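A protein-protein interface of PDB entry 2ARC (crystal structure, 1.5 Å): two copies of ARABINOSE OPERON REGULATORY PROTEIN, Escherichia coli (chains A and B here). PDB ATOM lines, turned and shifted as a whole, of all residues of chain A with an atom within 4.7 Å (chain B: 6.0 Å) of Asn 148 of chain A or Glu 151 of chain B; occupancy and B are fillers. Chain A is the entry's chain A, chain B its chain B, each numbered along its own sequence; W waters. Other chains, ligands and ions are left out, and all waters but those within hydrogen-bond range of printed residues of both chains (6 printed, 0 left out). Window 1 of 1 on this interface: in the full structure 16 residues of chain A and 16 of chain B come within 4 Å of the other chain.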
ATOM      1  N   LEU A 144     -17.869  26.055  -1.702  1.00  0.00           N
ATOM      2  CA  LEU A 144     -17.393  25.066  -0.734  1.00  0.00           C
ATOM      3  C   LEU A 144     -18.151  23.764  -0.892  1.00  0.00           C
ATOM      4  O   LEU A 144     -17.583  22.688  -0.716  1.00  0.00           O
ATOM      5  CB  LEU A 144     -17.590  25.569   0.691  1.00  0.00           C
ATOM      6  CG  LEU A 144     -16.651  26.658   1.153  1.00  0.00           C
ATOM      7  CD1 LEU A 144     -17.271  27.357   2.354  1.00  0.00           C
ATOM      8  CD2 LEU A 144     -15.307  26.047   1.463  1.00  0.00           C
ATOM      9  N   LEU A 145     -19.445  23.870  -1.184  1.00  0.00           N
ATOM     10  CA  LEU A 145     -20.295  22.706  -1.380  1.00  0.00           C
ATOM     11  C   LEU A 145     -19.847  21.957  -2.633  1.00  0.00           C
ATOM     12  O   LEU A 145     -19.767  20.725  -2.637  1.00  0.00           O
ATOM     13  CB  LEU A 145     -21.765  23.118  -1.537  1.00  0.00           C
ATOM     14  CG  LEU A 145     -22.788  22.626  -0.507  1.00  0.00           C
ATOM     15  CD1 LEU A 145     -24.182  22.827  -1.057  1.00  0.00           C
ATOM     16  CD2 LEU A 145     -22.562  21.158  -0.176  1.00  0.00           C
ATOM     17  N   ALA A 146     -19.555  22.706  -3.693  1.00  0.00           N
ATOM     18  CA  ALA A 146     -19.117  22.109  -4.956  1.00  0.00           C
ATOM     19  C   ALA A 146     -17.795  21.404  -4.759  1.00  0.00           C
ATOM     20  O   ALA A 146     -17.584  20.319  -5.304  1.00  0.00           O
ATOM     21  CB  ALA A 146     -19.007  23.174  -6.049  1.00  0.00           C
ATOM     22  N   ILE A 147     -16.913  22.015  -3.971  1.00  0.00           N
ATOM     23  CA  ILE A 147     -15.611  21.443  -3.649  1.00  0.00           C
ATOM     24  C   ILE A 147     -15.848  20.143  -2.859  1.00  0.00           C
ATOM     25  O   ILE A 147     -15.154  19.134  -3.035  1.00  0.00           O
ATOM     26  CB  ILE A 147     -14.789  22.423  -2.758  1.00  0.00           C
ATOM     27  CG1 ILE A 147     -14.325  23.641  -3.570  1.00  0.00           C
ATOM     28  CG2 ILE A 147     -13.607  21.709  -2.100  1.00  0.00           C
ATOM     29  CD1 ILE A 147     -13.149  23.366  -4.503  1.00  0.00           C
ATOM     30  N   ASN A 148     -16.819  20.197  -1.958  1.00  0.00           N
ATOM     31  CA  ASN A 148     -17.165  19.050  -1.140  1.00  0.00           C
ATOM     32  C   ASN A 148     -17.683  17.891  -1.985  1.00  0.00           C
ATOM     33  O   ASN A 148     -17.273  16.741  -1.805  1.00  0.00           O
ATOM     34  CB  ASN A 148     -18.234  19.445  -0.126  1.00  0.00           C
ATOM     35  CG  ASN A 148     -18.770  18.254   0.616  1.00  0.00           C
ATOM     36  OD1 ASN A 148     -18.132  17.755   1.557  1.00  0.00           O
ATOM     37  ND2 ASN A 148     -19.908  17.756   0.181  1.00  0.00           N
ATOM     38  N   LEU A 149     -18.594  18.195  -2.904  1.00  0.00           N
ATOM     39  CA  LEU A 149     -19.186  17.176  -3.779  1.00  0.00           C
ATOM     40  C   LEU A 149     -18.150  16.576  -4.733  1.00  0.00           C
ATOM     41  O   LEU A 149     -18.200  15.387  -5.078  1.00  0.00           O
ATOM     42  CB  LEU A 149     -20.367  17.764  -4.528  1.00  0.00           C
ATOM     43  CG  LEU A 149     -21.507  18.114  -3.570  1.00  0.00           C
ATOM     44  CD1 LEU A 149     -22.538  19.007  -4.251  1.00  0.00           C
ATOM     45  CD2 LEU A 149     -22.123  16.824  -3.068  1.00  0.00           C
ATOM     46  N   LEU A 150     -17.192  17.408  -5.108  1.00  0.00           N
ATOM     47  CA  LEU A 150     -16.087  17.012  -5.970  1.00  0.00           C
ATOM     48  C   LEU A 150     -15.212  16.018  -5.190  1.00  0.00           C
ATOM     49  O   LEU A 150     -14.833  14.959  -5.717  1.00  0.00           O
ATOM     50  CB  LEU A 150     -15.309  18.267  -6.360  1.00  0.00           C
ATOM     51  CG  LEU A 150     -14.130  18.199  -7.309  1.00  0.00           C
ATOM     52  CD1 LEU A 150     -14.419  17.285  -8.487  1.00  0.00           C
ATOM     53  CD2 LEU A 150     -13.856  19.614  -7.763  1.00  0.00           C
ATOM     54  N   GLU A 151     -14.892  16.341  -3.936  1.00  0.00           N
ATOM     55  CA  GLU A 151     -14.103  15.433  -3.111  1.00  0.00           C
ATOM     56  C   GLU A 151     -14.855  14.090  -2.993  1.00  0.00           C
ATOM     57  O   GLU A 151     -14.245  13.015  -3.041  1.00  0.00           O
ATOM     58  CB  GLU A 151     -13.873  16.032  -1.723  1.00  0.00           C
ATOM     59  CG  GLU A 151     -13.040  15.136  -0.799  1.00  0.00           C
ATOM     60  CD  GLU A 151     -12.861  15.744   0.576  1.00  0.00           C
ATOM     61  OE1 GLU A 151     -12.008  16.629   0.710  1.00  0.00           O
ATOM     62  OE2 GLU A 151     -13.604  15.357   1.510  1.00  0.00           O
ATOM     63  N   GLN A 152     -16.175  14.147  -2.845  1.00  0.00           N
ATOM     64  CA  GLN A 152     -16.952  12.922  -2.769  1.00  0.00           C
ATOM     65  C   GLN A 152     -16.764  12.073  -4.031  1.00  0.00           C
ATOM     66  O   GLN A 152     -16.586  10.867  -3.944  1.00  0.00           O
ATOM     67  CB  GLN A 152     -18.444  13.187  -2.586  1.00  0.00           C
ATOM     68  CG  GLN A 152     -19.171  11.895  -2.230  1.00  0.00           C
ATOM     69  CD  GLN A 152     -20.671  12.017  -2.223  1.00  0.00           C
ATOM     70  OE1 GLN A 152     -21.231  13.072  -1.889  1.00  0.00           O
ATOM     71  NE2 GLN A 152     -21.344  10.933  -2.588  1.00  0.00           N
ATOM     72  N   ARG B  95     -12.261  18.734  10.618  1.00  0.00           N
ATOM     73  CA  ARG B  95     -11.139  19.244   9.839  1.00  0.00           C
ATOM     74  C   ARG B  95     -11.022  20.705  10.327  1.00  0.00           C
ATOM     75  O   ARG B  95     -12.002  21.295  10.800  1.00  0.00           O
ATOM     76  CB  ARG B  95     -11.410  19.174   8.335  1.00  0.00           C
ATOM     77  CG  ARG B  95     -11.472  17.756   7.762  1.00  0.00           C
ATOM     78  CD  ARG B  95     -11.586  17.788   6.226  1.00  0.00           C
ATOM     79  NE  ARG B  95     -11.656  16.458   5.607  1.00  0.00           N
ATOM     80  CZ  ARG B  95     -10.599  15.671   5.390  1.00  0.00           C
ATOM     81  NH1 ARG B  95      -9.382  16.070   5.747  1.00  0.00           N
ATOM     82  NH2 ARG B  95     -10.738  14.494   4.789  1.00  0.00           N
ATOM     83  N   TYR B  97     -10.939  23.707   8.996  1.00  0.00           N
ATOM     84  CA  TYR B  97     -11.846  24.708   8.439  1.00  0.00           C
ATOM     85  C   TYR B  97     -13.350  24.536   8.719  1.00  0.00           C
ATOM     86  O   TYR B  97     -14.161  25.339   8.268  1.00  0.00           O
ATOM     87  CB  TYR B  97     -11.563  24.863   6.941  1.00  0.00           C
ATOM     88  CG  TYR B  97     -11.764  23.600   6.134  1.00  0.00           C
ATOM     89  CD1 TYR B  97     -10.718  22.682   5.956  1.00  0.00           C
ATOM     90  CD2 TYR B  97     -13.002  23.316   5.548  1.00  0.00           C
ATOM     91  CE1 TYR B  97     -10.901  21.520   5.217  1.00  0.00           C
ATOM     92  CE2 TYR B  97     -13.196  22.160   4.811  1.00  0.00           C
ATOM     93  CZ  TYR B  97     -12.144  21.262   4.646  1.00  0.00           C
ATOM     94  OH  TYR B  97     -12.345  20.125   3.905  1.00  0.00           O
ATOM     95  N   TRP B  98     -13.708  23.531   9.511  1.00  0.00           N
ATOM     96  CA  TRP B  98     -15.108  23.262   9.851  1.00  0.00           C
ATOM     97  C   TRP B  98     -15.657  24.101  10.998  1.00  0.00           C
ATOM     98  O   TRP B  98     -16.872  24.150  11.208  1.00  0.00           O
ATOM     99  CB  TRP B  98     -15.276  21.816  10.289  1.00  0.00           C
ATOM    100  CG  TRP B  98     -15.169  20.771   9.227  1.00  0.00           C
ATOM    101  CD1 TRP B  98     -14.742  20.929   7.939  1.00  0.00           C
ATOM    102  CD2 TRP B  98     -15.520  19.383   9.367  1.00  0.00           C
ATOM    103  NE1 TRP B  98     -14.816  19.726   7.270  1.00  0.00           N
ATOM    104  CE2 TRP B  98     -15.287  18.765   8.127  1.00  0.00           C
ATOM    105  CE3 TRP B  98     -16.010  18.610  10.435  1.00  0.00           C
ATOM    106  CZ2 TRP B  98     -15.532  17.395   7.917  1.00  0.00           C
ATOM    107  CZ3 TRP B  98     -16.249  17.259  10.227  1.00  0.00           C
ATOM    108  CH2 TRP B  98     -16.010  16.665   8.977  1.00  0.00           C
ATOM    109  N   TRP B 101     -18.723  26.298  10.743  1.00  0.00           N
ATOM    110  CA  TRP B 101     -19.942  25.507  10.555  1.00  0.00           C
ATOM    111  C   TRP B 101     -20.363  24.702  11.787  1.00  0.00           C
ATOM    112  O   TRP B 101     -21.359  23.976  11.741  1.00  0.00           O
ATOM    113  CB  TRP B 101     -19.779  24.578   9.353  1.00  0.00           C
ATOM    114  CG  TRP B 101     -19.021  25.216   8.208  1.00  0.00           C
ATOM    115  CD1 TRP B 101     -19.024  26.546   7.844  1.00  0.00           C
ATOM    116  CD2 TRP B 101     -18.157  24.553   7.278  1.00  0.00           C
ATOM    117  NE1 TRP B 101     -18.218  26.739   6.747  1.00  0.00           N
ATOM    118  CE2 TRP B 101     -17.673  25.537   6.380  1.00  0.00           C
ATOM    119  CE3 TRP B 101     -17.752  23.220   7.113  1.00  0.00           C
ATOM    120  CZ2 TRP B 101     -16.802  25.231   5.324  1.00  0.00           C
ATOM    121  CZ3 TRP B 101     -16.890  22.917   6.063  1.00  0.00           C
ATOM    122  CH2 TRP B 101     -16.425  23.918   5.184  1.00  0.00           C
ATOM    123  N   ALA B 146     -17.132   9.033   5.014  1.00  0.00           N
ATOM    124  CA  ALA B 146     -18.018   9.416   6.106  1.00  0.00           C
ATOM    125  C   ALA B 146     -17.712  10.873   6.498  1.00  0.00           C
ATOM    126  O   ALA B 146     -18.625  11.689   6.656  1.00  0.00           O
ATOM    127  CB  ALA B 146     -17.830   8.479   7.287  1.00  0.00           C
ATOM    128  N   ILE B 147     -16.427  11.201   6.611  1.00  0.00           N
ATOM    129  CA  ILE B 147     -15.987  12.560   6.944  1.00  0.00           C
ATOM    130  C   ILE B 147     -16.499  13.561   5.889  1.00  0.00           C
ATOM    131  O   ILE B 147     -17.002  14.649   6.223  1.00  0.00           O
ATOM    132  CB  ILE B 147     -14.441  12.628   7.024  1.00  0.00           C
ATOM    133  CG1 ILE B 147     -13.952  11.898   8.280  1.00  0.00           C
ATOM    134  CG2 ILE B 147     -13.946  14.071   7.013  1.00  0.00           C
ATOM    135  CD1 ILE B 147     -12.441  11.919   8.445  1.00  0.00           C
ATOM    136  N   ASN B 148     -16.378  13.179   4.620  1.00  0.00           N
ATOM    137  CA  ASN B 148     -16.822  14.007   3.515  1.00  0.00           C
ATOM    138  C   ASN B 148     -18.326  14.242   3.540  1.00  0.00           C
ATOM    139  O   ASN B 148     -18.794  15.358   3.277  1.00  0.00           O
ATOM    140  CB  ASN B 148     -16.433  13.359   2.180  1.00  0.00           C
ATOM    141  CG  ASN B 148     -17.046  14.066   0.998  1.00  0.00           C
ATOM    142  OD1 ASN B 148     -16.462  15.026   0.479  1.00  0.00           O
ATOM    143  ND2 ASN B 148     -18.228  13.616   0.572  1.00  0.00           N
ATOM    144  N   LEU B 149     -19.089  13.206   3.868  1.00  0.00           N
ATOM    145  CA  LEU B 149     -20.541  13.323   3.899  1.00  0.00           C
ATOM    146  C   LEU B 149     -20.963  14.205   5.070  1.00  0.00           C
ATOM    147  O   LEU B 149     -21.918  14.974   4.969  1.00  0.00           O
ATOM    148  CB  LEU B 149     -21.206  11.941   3.949  1.00  0.00           C
ATOM    149  CG  LEU B 149     -21.045  11.163   2.634  1.00  0.00           C
ATOM    150  CD1 LEU B 149     -21.291   9.651   2.822  1.00  0.00           C
ATOM    151  CD2 LEU B 149     -21.976  11.741   1.585  1.00  0.00           C
ATOM    152  N   LEU B 150     -20.228  14.104   6.171  1.00  0.00           N
ATOM    153  CA  LEU B 150     -20.495  14.910   7.350  1.00  0.00           C
ATOM    154  C   LEU B 150     -20.264  16.370   6.975  1.00  0.00           C
ATOM    155  O   LEU B 150     -21.084  17.231   7.292  1.00  0.00           O
ATOM    156  CB  LEU B 150     -19.571  14.499   8.492  1.00  0.00           C
ATOM    157  CG  LEU B 150     -19.664  15.267   9.814  1.00  0.00           C
ATOM    158  CD1 LEU B 150     -21.107  15.368  10.315  1.00  0.00           C
ATOM    159  CD2 LEU B 150     -18.773  14.544  10.838  1.00  0.00           C
ATOM    160  N   GLU B 151     -19.167  16.634   6.267  1.00  0.00           N
ATOM    161  CA  GLU B 151     -18.847  17.986   5.810  1.00  0.00           C
ATOM    162  C   GLU B 151     -19.980  18.509   4.920  1.00  0.00           C
ATOM    163  O   GLU B 151     -20.337  19.688   4.987  1.00  0.00           O
ATOM    164  CB  GLU B 151     -17.539  18.008   5.019  1.00  0.00           C
ATOM    165  CG  GLU B 151     -17.148  19.410   4.535  1.00  0.00           C
ATOM    166  CD  GLU B 151     -15.913  19.379   3.681  1.00  0.00           C
ATOM    167  OE1 GLU B 151     -14.804  19.377   4.252  1.00  0.00           O
ATOM    168  OE2 GLU B 151     -16.064  19.341   2.441  1.00  0.00           O
ATOM    169  N   GLN B 152     -20.541  17.630   4.093  1.00  0.00           N
ATOM    170  CA  GLN B 152     -21.645  18.011   3.219  1.00  0.00           C
ATOM    171  C   GLN B 152     -22.823  18.438   4.072  1.00  0.00           C
ATOM    172  O   GLN B 152     -23.463  19.456   3.789  1.00  0.00           O
ATOM    173  CB  GLN B 152     -22.085  16.864   2.290  1.00  0.00           C
ATOM    174  CG  GLN B 152     -23.036  17.349   1.200  1.00  0.00           C
ATOM    175  CD  GLN B 152     -23.762  16.241   0.449  1.00  0.00           C
ATOM    176  OE1 GLN B 152     -23.186  15.201   0.103  1.00  0.00           O
ATOM    177  NE2 GLN B 152     -25.031  16.468   0.181  1.00  0.00           N
ATOM    178  N   LEU B 153     -23.113  17.666   5.118  1.00  0.00           N
ATOM    179  CA  LEU B 153     -24.229  17.985   6.008  1.00  0.00           C
ATOM    180  C   LEU B 153     -24.006  19.344   6.680  1.00  0.00           C
ATOM    181  O   LEU B 153     -24.922  20.183   6.722  1.00  0.00           O
ATOM    182  CB  LEU B 153     -24.426  16.870   7.041  1.00  0.00           C
ATOM    183  CG  LEU B 153     -25.660  16.961   7.949  1.00  0.00           C
ATOM    184  CD1 LEU B 153     -26.055  15.575   8.401  1.00  0.00           C
ATOM    185  CD2 LEU B 153     -25.386  17.850   9.146  1.00  0.00           C
ATOM    186  N   LEU B 154     -22.784  19.591   7.163  1.00  0.00           N
ATOM    187  CA  LEU B 154     -22.482  20.875   7.799  1.00  0.00           C
ATOM    188  C   LEU B 154     -22.680  22.032   6.796  1.00  0.00           C
ATOM    189  O   LEU B 154     -23.252  23.081   7.138  1.00  0.00           O
ATOM    190  CB  LEU B 154     -21.067  20.884   8.381  1.00  0.00           C
ATOM    191  CG  LEU B 154     -20.822  19.913   9.555  1.00  0.00           C
ATOM    192  CD1 LEU B 154     -19.348  19.941   9.968  1.00  0.00           C
ATOM    193  CD2 LEU B 154     -21.727  20.220  10.759  1.00  0.00           C
ATOM    194  N   LEU B 155     -22.255  21.833   5.549  1.00  0.00           N
ATOM    195  CA  LEU B 155     -22.423  22.874   4.530  1.00  0.00           C
ATOM    196  C   LEU B 155     -23.896  23.099   4.125  1.00  0.00           C
ATOM    197  O   LEU B 155     -24.321  24.241   3.865  1.00  0.00           O
ATOM    198  CB  LEU B 155     -21.575  22.557   3.291  1.00  0.00           C
ATOM    199  CG  LEU B 155     -20.082  22.814   3.467  1.00  0.00           C
ATOM    200  CD1 LEU B 155     -19.327  22.151   2.330  1.00  0.00           C
ATOM    201  CD2 LEU B 155     -19.784  24.339   3.548  1.00  0.00           C
ATOM    202  N   ARG B 156     -24.661  22.014   4.064  1.00  0.00           N
ATOM    203  CA  ARG B 156     -26.074  22.097   3.718  1.00  0.00           C
ATOM    204  C   ARG B 156     -26.789  22.859   4.832  1.00  0.00           C
ATOM    205  O   ARG B 156     -27.769  23.556   4.580  1.00  0.00           O
ATOM    206  CB  ARG B 156     -26.672  20.703   3.553  1.00  0.00           C
ATOM    207  CG  ARG B 156     -26.045  19.881   2.432  1.00  0.00           C
ATOM    208  CD  ARG B 156     -26.723  20.150   1.125  1.00  0.00           C
ATOM    209  NE  ARG B 156     -26.191  19.347   0.028  1.00  0.00           N
ATOM    210  CZ  ARG B 156     -26.319  19.686  -1.251  1.00  0.00           C
ATOM    211  NH1 ARG B 156     -26.961  20.804  -1.572  1.00  0.00           N
ATOM    212  NH2 ARG B 156     -25.768  18.945  -2.206  1.00  0.00           N
HETATM  213  O   HOH W   1     -15.657  22.091   1.197  1.00  0.00           O
HETATM  214  O   HOH W   2     -24.360  13.239  -1.982  1.00  0.00           O
HETATM  215  O   HOH W   3     -12.703  13.346   3.253  1.00  0.00           O
HETATM  216  O   HOH W   4     -20.289  15.001  -0.199  1.00  0.00           O
HETATM  217  O   HOH W   5     -13.766  19.159   0.674  1.00  0.00           O
HETATM  218  O   HOH W   6     -14.162  16.490   4.082  1.00  0.00           O
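Of the printed residues of chain B, Leu 144 of chain A touches Trp 101 and Leu 155. Printed residues of chain B within 4 Å of Leu 145 of chain A: Leu 155 (3.9 Å) and Arg 156 (3.5 Å). Arg 95 of chain B touches none of the printed residues of chain A. Leu 150 of chain B touches none of the printed residues of chain A. Of chain A, only Asn 148 (2.8 Å) comes within 4 Å of Glu 151 of chain B. Printed residues of chain A within 4 Å of Arg 156 of chain B: Leu 145 and Leu 149. The nearest printed residue of chain B that does not touch Gln 152 of chain A is Glu 151 of chain B (7.4 Å).
Asn 148 of chain A touches Glu 151 of chain B, and with the chains exchanged Glu 151 of chain A touches Asn 148 of chain B. Asn 148 of chain A touches Gln 152 of chain B, and with the chains exchanged Gln 152 of chain A touches Asn 148 of chain B. Leu 149 of chain A touches Gln 152 of chain B, and with the chains exchanged Gln 152 of chain A touches Leu 149 of chain B. Gln 152 of chain B touches its own counterpart, Gln 152 of chain A.
Trp 101 of chain B touches Leu 144 of chain A (CZ2 to CD1, 3.7 Å). Leu 155 of chain B touches Leu 144 of chain A (CD1 to O, 3.6 Å). CD2 of Leu 145 of chain A touches CB of Leu 155 of chain B, at 3.9 Å. CD1 of Leu 145 of chain A touches NH1 of Arg 156 of chain B (3.5 Å). Leu 155 of chain B touches Asn 148 of chain A. Gln 152 of chain B touches Leu 149 of chain A (OE1 to CD2, 3.7 Å). Leu 149 of chain A touches Arg 156 of chain B. Gln 152 of chain A touches Leu 149 of chain B. OE1 of Gln 152 of chain B touches OE1 of Gln 152 of chain A, 3.5 Å away.
Water W4 lies within hydrogen-bond range of the side-chain amide nitrogen of Asn 148 of chain B (2.6 Å), the side-chain amide oxygen of Gln 152 of chain A (2.7 Å), the side-chain amide nitrogen of Asn 148 of chain A (2.8 Å) and the side-chain amide oxygen of Gln 152 of chain B (2.9 Å). Water W3 lies within hydrogen-bond range of the guanidinium group of Arg 95 of chain B (2.7 Å) and the side-chain carboxylate of Glu 151 of chain A (2.8 Å). Water W1 lies within hydrogen-bond range of the backbone carbonyl oxygen of Leu 144 of chain A (2.8 Å) and the side-chain carboxylate of Glu 151 of chain B (3.0 Å). Water W6 lies within hydrogen-bond range of the side-chain carboxylate of Glu 151 of chain A (2.9 Å), the guanidinium group of Arg 95 of chain B (2.9 Å) and the side-chain carboxylate of Glu 151 of chain B (3.0 Å). Water W5 lies within hydrogen-bond range of OE2 of Glu 151 of chain B (2.9 Å) and OE1 of Glu 151 of chain A (3.1 Å). Water W2 bridges the side-chain amide oxygen of Gln 152 of chain B (3.1 Å) and the side-chain amide oxygen of Gln 152 of chain A (3.1 Å).
The backbone carbonyl oxygen (O) of Asn 148 of chain A sits close to the side-chain amide oxygen (OD1) of Asn 148 of chain B, 3.0 Å away. The side-chain amide oxygen of Asn 148 of chain A lies close to the side-chain carboxylate of Glu 151 of chain B, 2.8 Å away. OD1 of Asn 148 of chain A sits close to N of Gln 152 of chain B (3.5 Å). The side-chain carboxylate (OE2) of Glu 151 of chain A lies close to the side-chain amide oxygen (OD1) of Asn 148 of chain B (3.1 Å). The backbone NH of Gln 152 of chain A lies within hydrogen-bond range of the side-chain amide oxygen of Asn 148 of chain B, at 3.5 Å.
The side-chain hydroxyl (OH) of Tyr 97 of chain B lies within hydrogen-bond range of the side-chain carboxylate (OE1) of Glu 151 of chain B (2.6 Å). NE1 of Trp 98 of chain B is in hydrogen-bond range of OE1 of Glu 151 of chain B (3.0 Å). The side-chain amide nitrogen (NE2) of Gln 152 of chain B sits close to the guanidinium group (NE) of Arg 156 of chain B (3.1 Å).
Hydrophobic or aromatic side chains of chain B that line the printed part of chain A: Trp 101, Leu 149 and Leu 155. Along chain B the printed residues that touch a printed residue of chain A span positions 101 to 156. Of the 9 printed residues of chain A, 6 touch a printed residue of chain B. Hydrophobic or aromatic side chains of chain A that line the printed part of chain B: Leu 144, Leu 145 and Leu 149. Among the printed residues, 14 pairs touch across the chains. Among the printed residues, no Asp or Glu carboxylate lies within 4 Å of a Lys or Arg side-chain nitrogen of the other chain.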
